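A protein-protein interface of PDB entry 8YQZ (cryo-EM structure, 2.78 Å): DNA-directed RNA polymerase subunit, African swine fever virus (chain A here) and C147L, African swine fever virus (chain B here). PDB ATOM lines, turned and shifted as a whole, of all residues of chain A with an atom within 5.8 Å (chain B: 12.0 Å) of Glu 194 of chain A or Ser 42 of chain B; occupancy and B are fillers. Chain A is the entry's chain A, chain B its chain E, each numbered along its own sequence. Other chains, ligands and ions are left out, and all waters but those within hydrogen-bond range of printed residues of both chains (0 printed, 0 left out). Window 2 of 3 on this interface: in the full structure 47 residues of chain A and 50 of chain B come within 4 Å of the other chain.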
ATOM      1  N   ASN A  19      -8.344  -6.543   5.723  1.00  0.00           N
ATOM      2  CA  ASN A  19      -7.474  -7.554   6.310  1.00  0.00           C
ATOM      3  C   ASN A  19      -6.889  -7.084   7.631  1.00  0.00           C
ATOM      4  O   ASN A  19      -6.704  -7.887   8.549  1.00  0.00           O
ATOM      5  CB  ASN A  19      -6.367  -7.918   5.331  1.00  0.00           C
ATOM      6  CG  ASN A  19      -6.857  -7.962   3.907  1.00  0.00           C
ATOM      7  OD1 ASN A  19      -7.509  -7.031   3.441  1.00  0.00           O
ATOM      8  ND2 ASN A  19      -6.545  -9.041   3.203  1.00  0.00           N
ATOM      9  N   ARG A 171     -15.504  -1.057  -5.683  1.00  0.00           N
ATOM     10  CA  ARG A 171     -14.483  -2.016  -5.278  1.00  0.00           C
ATOM     11  C   ARG A 171     -14.019  -2.863  -6.452  1.00  0.00           C
ATOM     12  O   ARG A 171     -12.818  -3.106  -6.614  1.00  0.00           O
ATOM     13  CB  ARG A 171     -15.021  -2.905  -4.162  1.00  0.00           C
ATOM     14  CG  ARG A 171     -14.301  -4.229  -4.011  1.00  0.00           C
ATOM     15  CD  ARG A 171     -14.851  -5.009  -2.835  1.00  0.00           C
ATOM     16  NE  ARG A 171     -14.327  -4.538  -1.560  1.00  0.00           N
ATOM     17  CZ  ARG A 171     -13.789  -5.326  -0.640  1.00  0.00           C
ATOM     18  NH1 ARG A 171     -13.699  -6.633  -0.817  1.00  0.00           N
ATOM     19  NH2 ARG A 171     -13.328  -4.789   0.485  1.00  0.00           N
ATOM     20  N   PHE A 174     -11.768  -0.757  -8.627  1.00  0.00           N
ATOM     21  CA  PHE A 174     -10.464  -0.469  -8.042  1.00  0.00           C
ATOM     22  C   PHE A 174      -9.600  -1.710  -7.910  1.00  0.00           C
ATOM     23  O   PHE A 174      -8.375  -1.588  -7.835  1.00  0.00           O
ATOM     24  CB  PHE A 174     -10.643   0.182  -6.673  1.00  0.00           C
ATOM     25  CG  PHE A 174     -11.014   1.630  -6.736  1.00  0.00           C
ATOM     26  CD1 PHE A 174     -10.822   2.357  -7.890  1.00  0.00           C
ATOM     27  CD2 PHE A 174     -11.581   2.255  -5.647  1.00  0.00           C
ATOM     28  CE1 PHE A 174     -11.169   3.680  -7.948  1.00  0.00           C
ATOM     29  CE2 PHE A 174     -11.931   3.577  -5.703  1.00  0.00           C
ATOM     30  CZ  PHE A 174     -11.726   4.290  -6.854  1.00  0.00           C
ATOM     31  N   SER A 175     -10.204  -2.897  -7.880  1.00  0.00           N
ATOM     32  CA  SER A 175      -9.418  -4.112  -7.722  1.00  0.00           C
ATOM     33  C   SER A 175      -8.592  -4.438  -8.954  1.00  0.00           C
ATOM     34  O   SER A 175      -7.691  -5.277  -8.873  1.00  0.00           O
ATOM     35  CB  SER A 175     -10.326  -5.290  -7.399  1.00  0.00           C
ATOM     36  OG  SER A 175      -9.637  -6.508  -7.595  1.00  0.00           O
ATOM     37  N   TYR A 179      -0.171  -2.308  -9.104  1.00  0.00           N
ATOM     38  CA  TYR A 179       0.648  -1.571  -8.146  1.00  0.00           C
ATOM     39  C   TYR A 179       1.559  -0.563  -8.833  1.00  0.00           C
ATOM     40  O   TYR A 179       1.972   0.418  -8.207  1.00  0.00           O
ATOM     41  CB  TYR A 179       1.477  -2.540  -7.306  1.00  0.00           C
ATOM     42  CG  TYR A 179       0.747  -3.076  -6.098  1.00  0.00           C
ATOM     43  CD1 TYR A 179       0.419  -2.248  -5.035  1.00  0.00           C
ATOM     44  CD2 TYR A 179       0.398  -4.413  -6.015  1.00  0.00           C
ATOM     45  CE1 TYR A 179      -0.244  -2.736  -3.934  1.00  0.00           C
ATOM     46  CE2 TYR A 179      -0.260  -4.910  -4.916  1.00  0.00           C
ATOM     47  CZ  TYR A 179      -0.581  -4.069  -3.878  1.00  0.00           C
ATOM     48  OH  TYR A 179      -1.241  -4.571  -2.781  1.00  0.00           O
ATOM     49  N   LYS A 189       2.749   1.955  -1.772  1.00  0.00           N
ATOM     50  CA  LYS A 189       2.158   0.632  -1.895  1.00  0.00           C
ATOM     51  C   LYS A 189       1.011   0.417  -0.919  1.00  0.00           C
ATOM     52  O   LYS A 189       0.033  -0.247  -1.270  1.00  0.00           O
ATOM     53  CB  LYS A 189       3.236  -0.431  -1.696  1.00  0.00           C
ATOM     54  CG  LYS A 189       2.706  -1.840  -1.568  1.00  0.00           C
ATOM     55  CD  LYS A 189       3.773  -2.865  -1.912  1.00  0.00           C
ATOM     56  CE  LYS A 189       3.180  -4.046  -2.660  1.00  0.00           C
ATOM     57  NZ  LYS A 189       2.895  -5.178  -1.743  1.00  0.00           N
ATOM     58  N   HIS A 192      -3.069   1.733  -1.630  1.00  0.00           N
ATOM     59  CA  HIS A 192      -3.789   1.211  -2.782  1.00  0.00           C
ATOM     60  C   HIS A 192      -5.267   1.575  -2.682  1.00  0.00           C
ATOM     61  O   HIS A 192      -5.855   1.486  -1.600  1.00  0.00           O
ATOM     62  CB  HIS A 192      -3.633  -0.306  -2.864  1.00  0.00           C
ATOM     63  CG  HIS A 192      -3.985  -0.880  -4.199  1.00  0.00           C
ATOM     64  ND1 HIS A 192      -5.287  -1.052  -4.613  1.00  0.00           N
ATOM     65  CD2 HIS A 192      -3.208  -1.353  -5.201  1.00  0.00           C
ATOM     66  CE1 HIS A 192      -5.298  -1.586  -5.821  1.00  0.00           C
ATOM     67  NE2 HIS A 192      -4.048  -1.783  -6.199  1.00  0.00           N
ATOM     68  N   PRO A 193      -5.899   1.984  -3.785  1.00  0.00           N
ATOM     69  CA  PRO A 193      -7.300   2.424  -3.706  1.00  0.00           C
ATOM     70  C   PRO A 193      -8.267   1.329  -3.300  1.00  0.00           C
ATOM     71  O   PRO A 193      -9.386   1.632  -2.872  1.00  0.00           O
ATOM     72  CB  PRO A 193      -7.590   2.925  -5.126  1.00  0.00           C
ATOM     73  CG  PRO A 193      -6.591   2.254  -5.975  1.00  0.00           C
ATOM     74  CD  PRO A 193      -5.359   2.136  -5.144  1.00  0.00           C
ATOM     75  N   GLU A 194      -7.880   0.061  -3.421  1.00  0.00           N
ATOM     76  CA  GLU A 194      -8.812  -1.016  -3.121  1.00  0.00           C
ATOM     77  C   GLU A 194      -9.137  -1.115  -1.638  1.00  0.00           C
ATOM     78  O   GLU A 194     -10.115  -1.773  -1.277  1.00  0.00           O
ATOM     79  CB  GLU A 194      -8.257  -2.346  -3.608  1.00  0.00           C
ATOM     80  CG  GLU A 194      -7.257  -2.964  -2.668  1.00  0.00           C
ATOM     81  CD  GLU A 194      -6.948  -4.391  -3.040  1.00  0.00           C
ATOM     82  OE1 GLU A 194      -7.539  -4.889  -4.021  1.00  0.00           O
ATOM     83  OE2 GLU A 194      -6.122  -5.020  -2.354  1.00  0.00           O
ATOM     84  N   LYS A 195      -8.339  -0.494  -0.771  1.00  0.00           N
ATOM     85  CA  LYS A 195      -8.644  -0.479   0.652  1.00  0.00           C
ATOM     86  C   LYS A 195      -9.670   0.580   1.007  1.00  0.00           C
ATOM     87  O   LYS A 195     -10.045   0.685   2.176  1.00  0.00           O
ATOM     88  CB  LYS A 195      -7.375  -0.255   1.468  1.00  0.00           C
ATOM     89  CG  LYS A 195      -6.297  -1.273   1.196  1.00  0.00           C
ATOM     90  CD  LYS A 195      -4.989  -0.911   1.870  1.00  0.00           C
ATOM     91  CE  LYS A 195      -4.933  -1.411   3.283  1.00  0.00           C
ATOM     92  NZ  LYS A 195      -3.529  -1.490   3.763  1.00  0.00           N
ATOM     93  N   LEU A 196     -10.120   1.366   0.035  1.00  0.00           N
ATOM     94  CA  LEU A 196     -11.089   2.421   0.283  1.00  0.00           C
ATOM     95  C   LEU A 196     -12.523   1.910   0.288  1.00  0.00           C
ATOM     96  O   LEU A 196     -13.445   2.705   0.486  1.00  0.00           O
ATOM     97  CB  LEU A 196     -10.931   3.537  -0.756  1.00  0.00           C
ATOM     98  CG  LEU A 196      -9.732   4.505  -0.730  1.00  0.00           C
ATOM     99  CD1 LEU A 196      -8.408   3.845  -0.407  1.00  0.00           C
ATOM    100  CD2 LEU A 196      -9.618   5.244  -2.052  1.00  0.00           C
ATOM    101  N   VAL A 197     -12.728   0.613   0.078  1.00  0.00           N
ATOM    102  CA  VAL A 197     -14.037  -0.021   0.176  1.00  0.00           C
ATOM    103  C   VAL A 197     -13.954  -1.102   1.242  1.00  0.00           C
ATOM    104  O   VAL A 197     -13.048  -1.942   1.211  1.00  0.00           O
ATOM    105  CB  VAL A 197     -14.486  -0.608  -1.175  1.00  0.00           C
ATOM    106  CG1 VAL A 197     -15.820  -1.304  -1.033  1.00  0.00           C
ATOM    107  CG2 VAL A 197     -14.573   0.489  -2.221  1.00  0.00           C
ATOM    108  N   SER B  42      -3.967  -4.868  -0.210  1.00  0.00           N
ATOM    109  CA  SER B  42      -4.301  -6.286  -0.107  1.00  0.00           C
ATOM    110  C   SER B  42      -3.769  -6.940   1.180  1.00  0.00           C
ATOM    111  O   SER B  42      -4.516  -7.647   1.853  1.00  0.00           O
ATOM    112  CB  SER B  42      -3.762  -7.043  -1.323  1.00  0.00           C
ATOM    113  OG  SER B  42      -2.346  -7.014  -1.355  1.00  0.00           O
ATOM    114  N   PRO B  43      -2.482  -6.729   1.534  1.00  0.00           N
ATOM    115  CA  PRO B  43      -2.000  -7.283   2.804  1.00  0.00           C
ATOM    116  C   PRO B  43      -2.251  -6.343   3.969  1.00  0.00           C
ATOM    117  O   PRO B  43      -2.851  -5.276   3.804  1.00  0.00           O
ATOM    118  CB  PRO B  43      -0.504  -7.476   2.548  1.00  0.00           C
ATOM    119  CG  PRO B  43      -0.165  -6.358   1.655  1.00  0.00           C
ATOM    120  CD  PRO B  43      -1.373  -6.104   0.785  1.00  0.00           C
ATOM    121  N   SER B  44      -1.801  -6.738   5.151  1.00  0.00           N
ATOM    122  CA  SER B  44      -1.875  -5.884   6.322  1.00  0.00           C
ATOM    123  C   SER B  44      -0.611  -5.035   6.420  1.00  0.00           C
ATOM    124  O   SER B  44       0.437  -5.377   5.869  1.00  0.00           O
ATOM    125  CB  SER B  44      -2.063  -6.727   7.584  1.00  0.00           C
ATOM    126  OG  SER B  44      -2.303  -5.912   8.717  1.00  0.00           O
ATOM    127  N   ILE B  45      -0.728  -3.906   7.124  1.00  0.00           N
ATOM    128  CA  ILE B  45       0.419  -3.015   7.281  1.00  0.00           C
ATOM    129  C   ILE B  45       1.540  -3.713   8.036  1.00  0.00           C
ATOM    130  O   ILE B  45       2.726  -3.459   7.790  1.00  0.00           O
ATOM    131  CB  ILE B  45      -0.001  -1.706   7.976  1.00  0.00           C
ATOM    132  CG1 ILE B  45      -1.348  -1.226   7.446  1.00  0.00           C
ATOM    133  CG2 ILE B  45       1.071  -0.634   7.808  1.00  0.00           C
ATOM    134  CD1 ILE B  45      -1.254  -0.539   6.105  1.00  0.00           C
ATOM    135  N   CYS B  46       1.184  -4.611   8.958  1.00  0.00           N
ATOM    136  CA  CYS B  46       2.179  -5.295   9.774  1.00  0.00           C
ATOM    137  C   CYS B  46       3.115  -6.167   8.950  1.00  0.00           C
ATOM    138  O   CYS B  46       4.255  -6.397   9.372  1.00  0.00           O
ATOM    139  CB  CYS B  46       1.487  -6.149  10.832  1.00  0.00           C
ATOM    140  SG  CYS B  46       0.686  -7.623  10.181  1.00  0.00           S
ATOM    141  N   GLU B  47       2.661  -6.662   7.795  1.00  0.00           N
ATOM    142  CA  GLU B  47       3.499  -7.524   6.968  1.00  0.00           C
ATOM    143  C   GLU B  47       4.715  -6.774   6.438  1.00  0.00           C
ATOM    144  O   GLU B  47       5.858  -7.217   6.602  1.00  0.00           O
ATOM    145  CB  GLU B  47       2.673  -8.099   5.818  1.00  0.00           C
ATOM    146  CG  GLU B  47       3.469  -8.937   4.831  1.00  0.00           C
ATOM    147  CD  GLU B  47       3.906  -8.140   3.613  1.00  0.00           C
ATOM    148  OE1 GLU B  47       3.173  -7.210   3.217  1.00  0.00           O
ATOM    149  OE2 GLU B  47       4.980  -8.439   3.054  1.00  0.00           O
ATOM    150  N   GLY B  48       4.487  -5.626   5.804  1.00  0.00           N
ATOM    151  CA  GLY B  48       5.580  -4.851   5.249  1.00  0.00           C
ATOM    152  C   GLY B  48       6.368  -4.040   6.251  1.00  0.00           C
ATOM    153  O   GLY B  48       7.409  -3.480   5.890  1.00  0.00           O
ATOM    154  N   PHE B  49       5.901  -3.961   7.494  1.00  0.00           N
ATOM    155  CA  PHE B  49       6.621  -3.224   8.522  1.00  0.00           C
ATOM    156  C   PHE B  49       7.914  -3.940   8.876  1.00  0.00           C
ATOM    157  O   PHE B  49       7.928  -5.155   9.084  1.00  0.00           O
ATOM    158  CB  PHE B  49       5.745  -3.054   9.760  1.00  0.00           C
ATOM    159  CG  PHE B  49       6.427  -2.356  10.897  1.00  0.00           C
ATOM    160  CD1 PHE B  49       6.462  -0.980  10.964  1.00  0.00           C
ATOM    161  CD2 PHE B  49       7.010  -3.078  11.917  1.00  0.00           C
ATOM    162  CE1 PHE B  49       7.086  -0.343  12.019  1.00  0.00           C
ATOM    163  CE2 PHE B  49       7.634  -2.447  12.965  1.00  0.00           C
ATOM    164  CZ  PHE B  49       7.669  -1.081  13.017  1.00  0.00           C
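The side-chain hydroxyl of Ser 42 of chain B sits at hydrogen-bond distance from the side-chain hydroxyl of Tyr 179 of chain A (3.0 Å).
The side-chain amide nitrogen (ND2) of Asn 19 of chain A is in hydrogen-bond range of the backbone carbonyl oxygen (O) of Ser 42 of chain B.
OE2 of Glu 194 of chain A sits at hydrogen-bond distance from N of Ser 42 of chain B (3.0 Å).
A ring nitrogen (ND1) of His 192 of chain A is in hydrogen-bond range of the backbone NH (N) of Glu 194 of chain A, at 3.1 Å.
Among the printed residues, pairs that only touch across the chains: Lys 195 of chain A with Ile 45 of chain B (3.4 Å), Lys 195 of chain A with Pro 43 of chain B (3.8 Å) and Tyr 179 of chain A with Pro 43 of chain B (3.9 Å).
Of chain B, only Ser 42 (3.0 Å) comes within 4 Å of Glu 194 of chain A.
Ser 42 of chain B touches three residues of chain A.
No residue of chain B comes within 4 Å of Arg 171 of chain A.
Ser 175 of chain A touches none of the printed residues of chain B.
No residue of chain B comes within 4 Å of Pro 193 of chain A.
No residue of chain B comes within 4 Å of Leu 196 of chain A.
No residue of chain B comes within 4 Å of Val 197 of chain A.
Printed residues of chain A within 4 Å of Pro 43 of chain B: Tyr 179 and Lys 195.
Of the printed residues of chain A, Ile 45 of chain B touches Lys 195.
Glu 47 of chain B touches none of the printed residues of chain A.
Cys 46 of chain B touches none of the printed residues of chain A.
The nearest residue of chain B that does not touch Glu 194 of chain A is Pro 43 of chain B (5.6 Å).
The nearest residue of chain A that does not touch Ser 42 of chain B is Lys 195 of chain A (4.5 Å).
The nearest printed residue of chain A that does not touch Pro 43 of chain B is Asn 19 of chain A (4.6 Å).
Of the 8 printed residues of chain B, 3 touch a printed residue of chain A.
Printed residues of chain B that touch a printed residue of chain A: Ser 42, Pro 43 and Ile 45.
Of the 12 printed residues of chain A, 4 touch a printed residue of chain B.
Hydrophobic or aromatic side chains of chain A within 4 Å of the printed part of chain B: Tyr 179.
Among the printed residues, 6 pairs touch across the chains.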
